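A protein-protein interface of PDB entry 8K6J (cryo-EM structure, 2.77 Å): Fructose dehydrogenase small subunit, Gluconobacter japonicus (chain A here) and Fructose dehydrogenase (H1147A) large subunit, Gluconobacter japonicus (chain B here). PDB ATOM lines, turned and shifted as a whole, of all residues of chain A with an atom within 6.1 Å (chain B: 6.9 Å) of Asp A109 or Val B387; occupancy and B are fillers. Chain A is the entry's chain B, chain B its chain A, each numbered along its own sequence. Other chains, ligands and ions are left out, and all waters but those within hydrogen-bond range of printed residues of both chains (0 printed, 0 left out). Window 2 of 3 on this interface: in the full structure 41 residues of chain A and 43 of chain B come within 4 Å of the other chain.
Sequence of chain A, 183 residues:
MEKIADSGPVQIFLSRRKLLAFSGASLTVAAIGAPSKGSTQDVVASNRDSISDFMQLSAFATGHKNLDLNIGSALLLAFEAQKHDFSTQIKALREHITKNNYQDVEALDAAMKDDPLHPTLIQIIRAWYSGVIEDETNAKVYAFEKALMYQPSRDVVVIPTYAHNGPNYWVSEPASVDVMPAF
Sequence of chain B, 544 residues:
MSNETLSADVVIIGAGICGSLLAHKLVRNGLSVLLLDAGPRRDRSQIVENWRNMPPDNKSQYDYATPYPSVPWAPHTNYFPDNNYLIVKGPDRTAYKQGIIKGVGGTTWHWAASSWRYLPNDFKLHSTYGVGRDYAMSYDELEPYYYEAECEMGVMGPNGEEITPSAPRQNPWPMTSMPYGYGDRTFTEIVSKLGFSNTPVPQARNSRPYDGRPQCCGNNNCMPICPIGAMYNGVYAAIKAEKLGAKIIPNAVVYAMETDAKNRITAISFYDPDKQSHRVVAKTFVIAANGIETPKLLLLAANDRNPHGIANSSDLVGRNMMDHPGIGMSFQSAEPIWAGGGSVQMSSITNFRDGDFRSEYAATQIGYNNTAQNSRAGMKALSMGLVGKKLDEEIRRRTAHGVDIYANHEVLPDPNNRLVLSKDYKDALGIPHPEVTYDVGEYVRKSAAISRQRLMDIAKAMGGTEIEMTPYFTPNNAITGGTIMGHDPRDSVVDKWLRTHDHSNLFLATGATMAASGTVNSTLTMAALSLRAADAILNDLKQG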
ATOM      1  N   ALA A  61      -6.156  -8.488 -12.481  1.00  0.00           N
ATOM      2  CA  ALA A  61      -7.169  -8.453 -13.529  1.00  0.00           C
ATOM      3  C   ALA A  61      -8.575  -8.526 -12.949  1.00  0.00           C
ATOM      4  O   ALA A  61      -9.449  -7.731 -13.313  1.00  0.00           O
ATOM      5  CB  ALA A  61      -6.937  -9.595 -14.517  1.00  0.00           C
ATOM      6  N   ASP A 104      -5.463   0.007 -11.869  1.00  0.00           N
ATOM      7  CA  ASP A 104      -6.437  -1.071 -11.808  1.00  0.00           C
ATOM      8  C   ASP A 104      -6.638  -1.635 -13.205  1.00  0.00           C
ATOM      9  O   ASP A 104      -6.091  -1.131 -14.188  1.00  0.00           O
ATOM     10  CB  ASP A 104      -7.770  -0.593 -11.221  1.00  0.00           C
ATOM     11  CG  ASP A 104      -8.170   0.778 -11.726  1.00  0.00           C
ATOM     12  OD1 ASP A 104      -7.720   1.164 -12.825  1.00  0.00           O
ATOM     13  OD2 ASP A 104      -8.936   1.471 -11.023  1.00  0.00           O
ATOM     14  N   VAL A 105      -7.442  -2.699 -13.288  1.00  0.00           N
ATOM     15  CA  VAL A 105      -7.684  -3.332 -14.578  1.00  0.00           C
ATOM     16  C   VAL A 105      -8.556  -2.463 -15.473  1.00  0.00           C
ATOM     17  O   VAL A 105      -8.594  -2.680 -16.688  1.00  0.00           O
ATOM     18  CB  VAL A 105      -8.303  -4.729 -14.389  1.00  0.00           C
ATOM     19  CG1 VAL A 105      -9.787  -4.629 -14.117  1.00  0.00           C
ATOM     20  CG2 VAL A 105      -8.036  -5.596 -15.608  1.00  0.00           C
ATOM     21  N   GLU A 106      -9.254  -1.471 -14.912  1.00  0.00           N
ATOM     22  CA  GLU A 106     -10.002  -0.540 -15.750  1.00  0.00           C
ATOM     23  C   GLU A 106      -9.070   0.205 -16.697  1.00  0.00           C
ATOM     24  O   GLU A 106      -9.318   0.275 -17.906  1.00  0.00           O
ATOM     25  CB  GLU A 106     -10.785   0.454 -14.885  1.00  0.00           C
ATOM     26  CG  GLU A 106     -12.112  -0.040 -14.280  1.00  0.00           C
ATOM     27  CD  GLU A 106     -11.984  -1.213 -13.313  1.00  0.00           C
ATOM     28  OE1 GLU A 106     -12.952  -1.457 -12.563  1.00  0.00           O
ATOM     29  OE2 GLU A 106     -10.928  -1.871 -13.263  1.00  0.00           O
ATOM     30  N   ALA A 107      -7.983   0.762 -16.160  1.00  0.00           N
ATOM     31  CA  ALA A 107      -7.029   1.486 -16.995  1.00  0.00           C
ATOM     32  C   ALA A 107      -6.313   0.551 -17.960  1.00  0.00           C
ATOM     33  O   ALA A 107      -6.079   0.908 -19.120  1.00  0.00           O
ATOM     34  CB  ALA A 107      -6.022   2.227 -16.117  1.00  0.00           C
ATOM     35  N   LEU A 108      -5.950  -0.648 -17.498  1.00  0.00           N
ATOM     36  CA  LEU A 108      -5.266  -1.599 -18.368  1.00  0.00           C
ATOM     37  C   LEU A 108      -6.151  -2.013 -19.535  1.00  0.00           C
ATOM     38  O   LEU A 108      -5.663  -2.212 -20.653  1.00  0.00           O
ATOM     39  CB  LEU A 108      -4.827  -2.823 -17.565  1.00  0.00           C
ATOM     40  CG  LEU A 108      -4.455  -4.072 -18.366  1.00  0.00           C
ATOM     41  CD1 LEU A 108      -3.058  -3.939 -18.944  1.00  0.00           C
ATOM     42  CD2 LEU A 108      -4.561  -5.315 -17.503  1.00  0.00           C
ATOM     43  N   ASP A 109      -7.454  -2.159 -19.293  1.00  0.00           N
ATOM     44  CA  ASP A 109      -8.370  -2.509 -20.372  1.00  0.00           C
ATOM     45  C   ASP A 109      -8.625  -1.321 -21.290  1.00  0.00           C
ATOM     46  O   ASP A 109      -8.719  -1.485 -22.512  1.00  0.00           O
ATOM     47  CB  ASP A 109      -9.679  -3.039 -19.789  1.00  0.00           C
ATOM     48  CG  ASP A 109     -10.824  -2.993 -20.781  1.00  0.00           C
ATOM     49  OD1 ASP A 109     -11.490  -1.940 -20.878  1.00  0.00           O
ATOM     50  OD2 ASP A 109     -11.062  -4.012 -21.460  1.00  0.00           O
ATOM     51  N   ALA A 110      -8.750  -0.116 -20.724  1.00  0.00           N
ATOM     52  CA  ALA A 110      -8.980   1.068 -21.547  1.00  0.00           C
ATOM     53  C   ALA A 110      -7.807   1.312 -22.485  1.00  0.00           C
ATOM     54  O   ALA A 110      -7.991   1.535 -23.687  1.00  0.00           O
ATOM     55  CB  ALA A 110      -9.226   2.286 -20.658  1.00  0.00           C
ATOM     56  N   ALA A 111      -6.590   1.269 -21.954  1.00  0.00           N
ATOM     57  CA  ALA A 111      -5.405   1.264 -22.791  1.00  0.00           C
ATOM     58  C   ALA A 111      -5.160  -0.154 -23.297  1.00  0.00           C
ATOM     59  O   ALA A 111      -5.953  -1.068 -23.061  1.00  0.00           O
ATOM     60  CB  ALA A 111      -4.202   1.802 -22.020  1.00  0.00           C
ATOM     61  N   MET A 112      -4.068  -0.339 -24.035  1.00  0.00           N
ATOM     62  CA  MET A 112      -3.623  -1.647 -24.506  1.00  0.00           C
ATOM     63  C   MET A 112      -4.666  -2.331 -25.390  1.00  0.00           C
ATOM     64  O   MET A 112      -4.470  -3.474 -25.813  1.00  0.00           O
ATOM     65  CB  MET A 112      -3.212  -2.532 -23.311  1.00  0.00           C
ATOM     66  CG  MET A 112      -2.531  -3.865 -23.621  1.00  0.00           C
ATOM     67  SD  MET A 112      -3.268  -5.279 -22.771  1.00  0.00           S
ATOM     68  CE  MET A 112      -4.933  -5.288 -23.416  1.00  0.00           C
ATOM     69  N   LYS A 113      -5.752  -1.638 -25.725  1.00  0.00           N
ATOM     70  CA  LYS A 113      -6.767  -2.203 -26.601  1.00  0.00           C
ATOM     71  C   LYS A 113      -6.188  -2.443 -27.989  1.00  0.00           C
ATOM     72  O   LYS A 113      -5.302  -1.713 -28.442  1.00  0.00           O
ATOM     73  CB  LYS A 113      -7.974  -1.271 -26.687  1.00  0.00           C
ATOM     74  CG  LYS A 113      -9.304  -1.988 -26.895  1.00  0.00           C
ATOM     75  CD  LYS A 113     -10.513  -1.103 -26.578  1.00  0.00           C
ATOM     76  CE  LYS A 113     -10.354   0.355 -27.017  1.00  0.00           C
ATOM     77  NZ  LYS A 113      -9.755   0.534 -28.377  1.00  0.00           N
ATOM     78  N   HIS A 118      -4.849  -8.569 -25.371  1.00  0.00           N
ATOM     79  CA  HIS A 118      -6.214  -8.423 -24.868  1.00  0.00           C
ATOM     80  C   HIS A 118      -6.968  -9.745 -24.799  1.00  0.00           C
ATOM     81  O   HIS A 118      -7.619 -10.002 -23.769  1.00  0.00           O
ATOM     82  CB  HIS A 118      -6.968  -7.394 -25.716  1.00  0.00           C
ATOM     83  CG  HIS A 118      -8.106  -6.739 -24.999  1.00  0.00           C
ATOM     84  ND1 HIS A 118      -9.350  -6.578 -25.568  1.00  0.00           N
ATOM     85  CD2 HIS A 118      -8.189  -6.205 -23.758  1.00  0.00           C
ATOM     86  CE1 HIS A 118     -10.150  -5.971 -24.710  1.00  0.00           C
ATOM     87  NE2 HIS A 118      -9.469  -5.734 -23.603  1.00  0.00           N
ATOM     88  N   LEU A 121      -5.993 -11.758 -21.663  1.00  0.00           N
ATOM     89  CA  LEU A 121      -6.466 -11.127 -20.435  1.00  0.00           C
ATOM     90  C   LEU A 121      -7.961 -11.350 -20.242  1.00  0.00           C
ATOM     91  O   LEU A 121      -8.413 -11.679 -19.135  1.00  0.00           O
ATOM     92  CB  LEU A 121      -6.145  -9.635 -20.455  1.00  0.00           C
ATOM     93  CG  LEU A 121      -6.886  -8.781 -19.429  1.00  0.00           C
ATOM     94  CD1 LEU A 121      -6.226  -8.907 -18.072  1.00  0.00           C
ATOM     95  CD2 LEU A 121      -6.925  -7.331 -19.869  1.00  0.00           C
ATOM     96  N   ILE A 122      -8.743 -11.178 -21.309  1.00  0.00           N
ATOM     97  CA  ILE A 122     -10.179 -11.422 -21.215  1.00  0.00           C
ATOM     98  C   ILE A 122     -10.447 -12.886 -20.899  1.00  0.00           C
ATOM     99  O   ILE A 122     -11.365 -13.215 -20.141  1.00  0.00           O
ATOM    100  CB  ILE A 122     -10.886 -10.974 -22.506  1.00  0.00           C
ATOM    101  CG1 ILE A 122     -10.688  -9.474 -22.722  1.00  0.00           C
ATOM    102  CG2 ILE A 122     -12.365 -11.304 -22.448  1.00  0.00           C
ATOM    103  CD1 ILE A 122     -11.314  -8.618 -21.649  1.00  0.00           C
ATOM    104  N   ILE A 125      -9.838 -13.399 -17.176  1.00  0.00           N
ATOM    105  CA  ILE A 125     -10.941 -12.858 -16.386  1.00  0.00           C
ATOM    106  C   ILE A 125     -12.161 -13.766 -16.480  1.00  0.00           C
ATOM    107  O   ILE A 125     -12.816 -14.059 -15.471  1.00  0.00           O
ATOM    108  CB  ILE A 125     -11.265 -11.423 -16.835  1.00  0.00           C
ATOM    109  CG1 ILE A 125     -10.236 -10.450 -16.268  1.00  0.00           C
ATOM    110  CG2 ILE A 125     -12.658 -11.026 -16.395  1.00  0.00           C
ATOM    111  CD1 ILE A 125     -10.377  -9.051 -16.796  1.00  0.00           C
ATOM    112  N   ALA B 381     -22.942 -10.920 -18.562  1.00  0.00           N
ATOM    113  CA  ALA B 381     -22.029  -9.819 -18.282  1.00  0.00           C
ATOM    114  C   ALA B 381     -20.632 -10.110 -18.809  1.00  0.00           C
ATOM    115  O   ALA B 381     -19.957  -9.210 -19.318  1.00  0.00           O
ATOM    116  CB  ALA B 381     -21.990  -9.536 -16.784  1.00  0.00           C
ATOM    117  N   GLY B 385     -17.930  -8.181 -22.401  1.00  0.00           N
ATOM    118  CA  GLY B 385     -16.569  -7.677 -22.353  1.00  0.00           C
ATOM    119  C   GLY B 385     -16.337  -6.588 -21.328  1.00  0.00           C
ATOM    120  O   GLY B 385     -15.638  -5.609 -21.618  1.00  0.00           O
ATOM    121  N   LEU B 386     -16.907  -6.731 -20.136  1.00  0.00           N
ATOM    122  CA  LEU B 386     -16.705  -5.784 -19.052  1.00  0.00           C
ATOM    123  C   LEU B 386     -15.622  -6.295 -18.113  1.00  0.00           C
ATOM    124  O   LEU B 386     -15.373  -7.499 -18.021  1.00  0.00           O
ATOM    125  CB  LEU B 386     -18.004  -5.554 -18.280  1.00  0.00           C
ATOM    126  CG  LEU B 386     -19.065  -4.735 -19.013  1.00  0.00           C
ATOM    127  CD1 LEU B 386     -20.429  -4.967 -18.401  1.00  0.00           C
ATOM    128  CD2 LEU B 386     -18.710  -3.259 -18.987  1.00  0.00           C
ATOM    129  N   VAL B 387     -14.973  -5.365 -17.416  1.00  0.00           N
ATOM    130  CA  VAL B 387     -13.821  -5.680 -16.579  1.00  0.00           C
ATOM    131  C   VAL B 387     -13.924  -4.917 -15.268  1.00  0.00           C
ATOM    132  O   VAL B 387     -14.445  -3.798 -15.224  1.00  0.00           O
ATOM    133  CB  VAL B 387     -12.498  -5.339 -17.292  1.00  0.00           C
ATOM    134  CG1 VAL B 387     -12.211  -6.343 -18.393  1.00  0.00           C
ATOM    135  CG2 VAL B 387     -12.559  -3.932 -17.852  1.00  0.00           C
ATOM    136  N   GLY B 388     -13.428  -5.531 -14.195  1.00  0.00           N
ATOM    137  CA  GLY B 388     -13.260  -4.810 -12.945  1.00  0.00           C
ATOM    138  C   GLY B 388     -14.574  -4.528 -12.243  1.00  0.00           C
ATOM    139  O   GLY B 388     -15.483  -5.364 -12.204  1.00  0.00           O
ATOM    140  N   LYS B 389     -14.667  -3.326 -11.671  1.00  0.00           N
ATOM    141  CA  LYS B 389     -15.838  -2.959 -10.881  1.00  0.00           C
ATOM    142  C   LYS B 389     -17.099  -2.936 -11.734  1.00  0.00           C
ATOM    143  O   LYS B 389     -18.182  -3.316 -11.268  1.00  0.00           O
ATOM    144  CB  LYS B 389     -15.612  -1.602 -10.220  1.00  0.00           C
ATOM    145  CG  LYS B 389     -16.685  -1.204  -9.226  1.00  0.00           C
ATOM    146  CD  LYS B 389     -16.519   0.242  -8.791  1.00  0.00           C
ATOM    147  CE  LYS B 389     -15.097   0.525  -8.333  1.00  0.00           C
ATOM    148  NZ  LYS B 389     -14.652  -0.423  -7.273  1.00  0.00           N
ATOM    149  N   LYS B 390     -16.982  -2.481 -12.983  1.00  0.00           N
ATOM    150  CA  LYS B 390     -18.139  -2.452 -13.868  1.00  0.00           C
ATOM    151  C   LYS B 390     -18.694  -3.850 -14.092  1.00  0.00           C
ATOM    152  O   LYS B 390     -19.913  -4.038 -14.159  1.00  0.00           O
ATOM    153  CB  LYS B 390     -17.766  -1.804 -15.200  1.00  0.00           C
ATOM    154  CG  LYS B 390     -17.143  -0.431 -15.064  1.00  0.00           C
ATOM    155  CD  LYS B 390     -18.104   0.651 -15.519  1.00  0.00           C
ATOM    156  CE  LYS B 390     -18.740   1.353 -14.334  1.00  0.00           C
ATOM    157  NZ  LYS B 390     -19.686   2.419 -14.762  1.00  0.00           N
ATOM    158  N   LEU B 391     -17.814  -4.846 -14.210  1.00  0.00           N
ATOM    159  CA  LEU B 391     -18.275  -6.216 -14.399  1.00  0.00           C
ATOM    160  C   LEU B 391     -19.080  -6.701 -13.199  1.00  0.00           C
ATOM    161  O   LEU B 391     -20.138  -7.317 -13.363  1.00  0.00           O
ATOM    162  CB  LEU B 391     -17.083  -7.138 -14.652  1.00  0.00           C
ATOM    163  CG  LEU B 391     -17.397  -8.627 -14.774  1.00  0.00           C
ATOM    164  CD1 LEU B 391     -18.439  -8.865 -15.847  1.00  0.00           C
ATOM    165  CD2 LEU B 391     -16.134  -9.411 -15.072  1.00  0.00           C
ATOM    166  N   ASP B 392     -18.596  -6.429 -11.985  1.00  0.00           N
ATOM    167  CA  ASP B 392     -19.328  -6.841 -10.792  1.00  0.00           C
ATOM    168  C   ASP B 392     -20.668  -6.123 -10.693  1.00  0.00           C
ATOM    169  O   ASP B 392     -21.688  -6.739 -10.358  1.00  0.00           O
ATOM    170  CB  ASP B 392     -18.489  -6.579  -9.543  1.00  0.00           C
ATOM    171  CG  ASP B 392     -17.186  -7.346  -9.548  1.00  0.00           C
ATOM    172  OD1 ASP B 392     -17.104  -8.372 -10.252  1.00  0.00           O
ATOM    173  OD2 ASP B 392     -16.245  -6.924  -8.845  1.00  0.00           O
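The backbone NH (N) of Lys B389 is in hydrogen-bond range of the side-chain carboxylate (OE1) of Glu A106.
OD2 of Asp A109 sits at hydrogen-bond distance from NE2 of His A118, 3.2 Å away.
Among the printed residues, merely in contact across the chains: Glu A106 with Gly B388 (3.4 Å), Asp A109 with Val B387 (3.5 Å), Ile A125 with Val B387 (3.6 Å), Val A105 with Gly B388 (3.7 Å) and Glu A106 with Val B387 (3.8 Å).
Of chain B, only Val B387 (3.5 Å) comes within 4 Å of Asp A109. Ala A110 touches none of the printed residues of chain B. Of the printed residues of chain B, Ile A125 touches Val B387 (3.6 Å). Val B387 touches just these residues of chain A: Glu A106, Asp A109 and Ile A125. Of the printed residues of chain A, Gly B388 touches Val A105 (3.7 Å) and Glu A106 (3.4 Å). The nearest residue of chain B that does not touch Asp A109 is Gly B385 (4.8 Å). The nearest residue of chain A that does not touch Val B387 is Ile A122 (4.1 Å). The nearest printed residue of chain B that does not touch Val A105 is Val B387 (4.2 Å).
Of the 9 printed residues of chain B, 3 touch a printed residue of chain A. Hydrophobic or aromatic side chains of chain B within 4 Å of the printed part of chain A: Val B387. Among the printed residues, no Asp or Glu carboxylate lies within 4 Å of a Lys or Arg side-chain nitrogen of the other chain.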
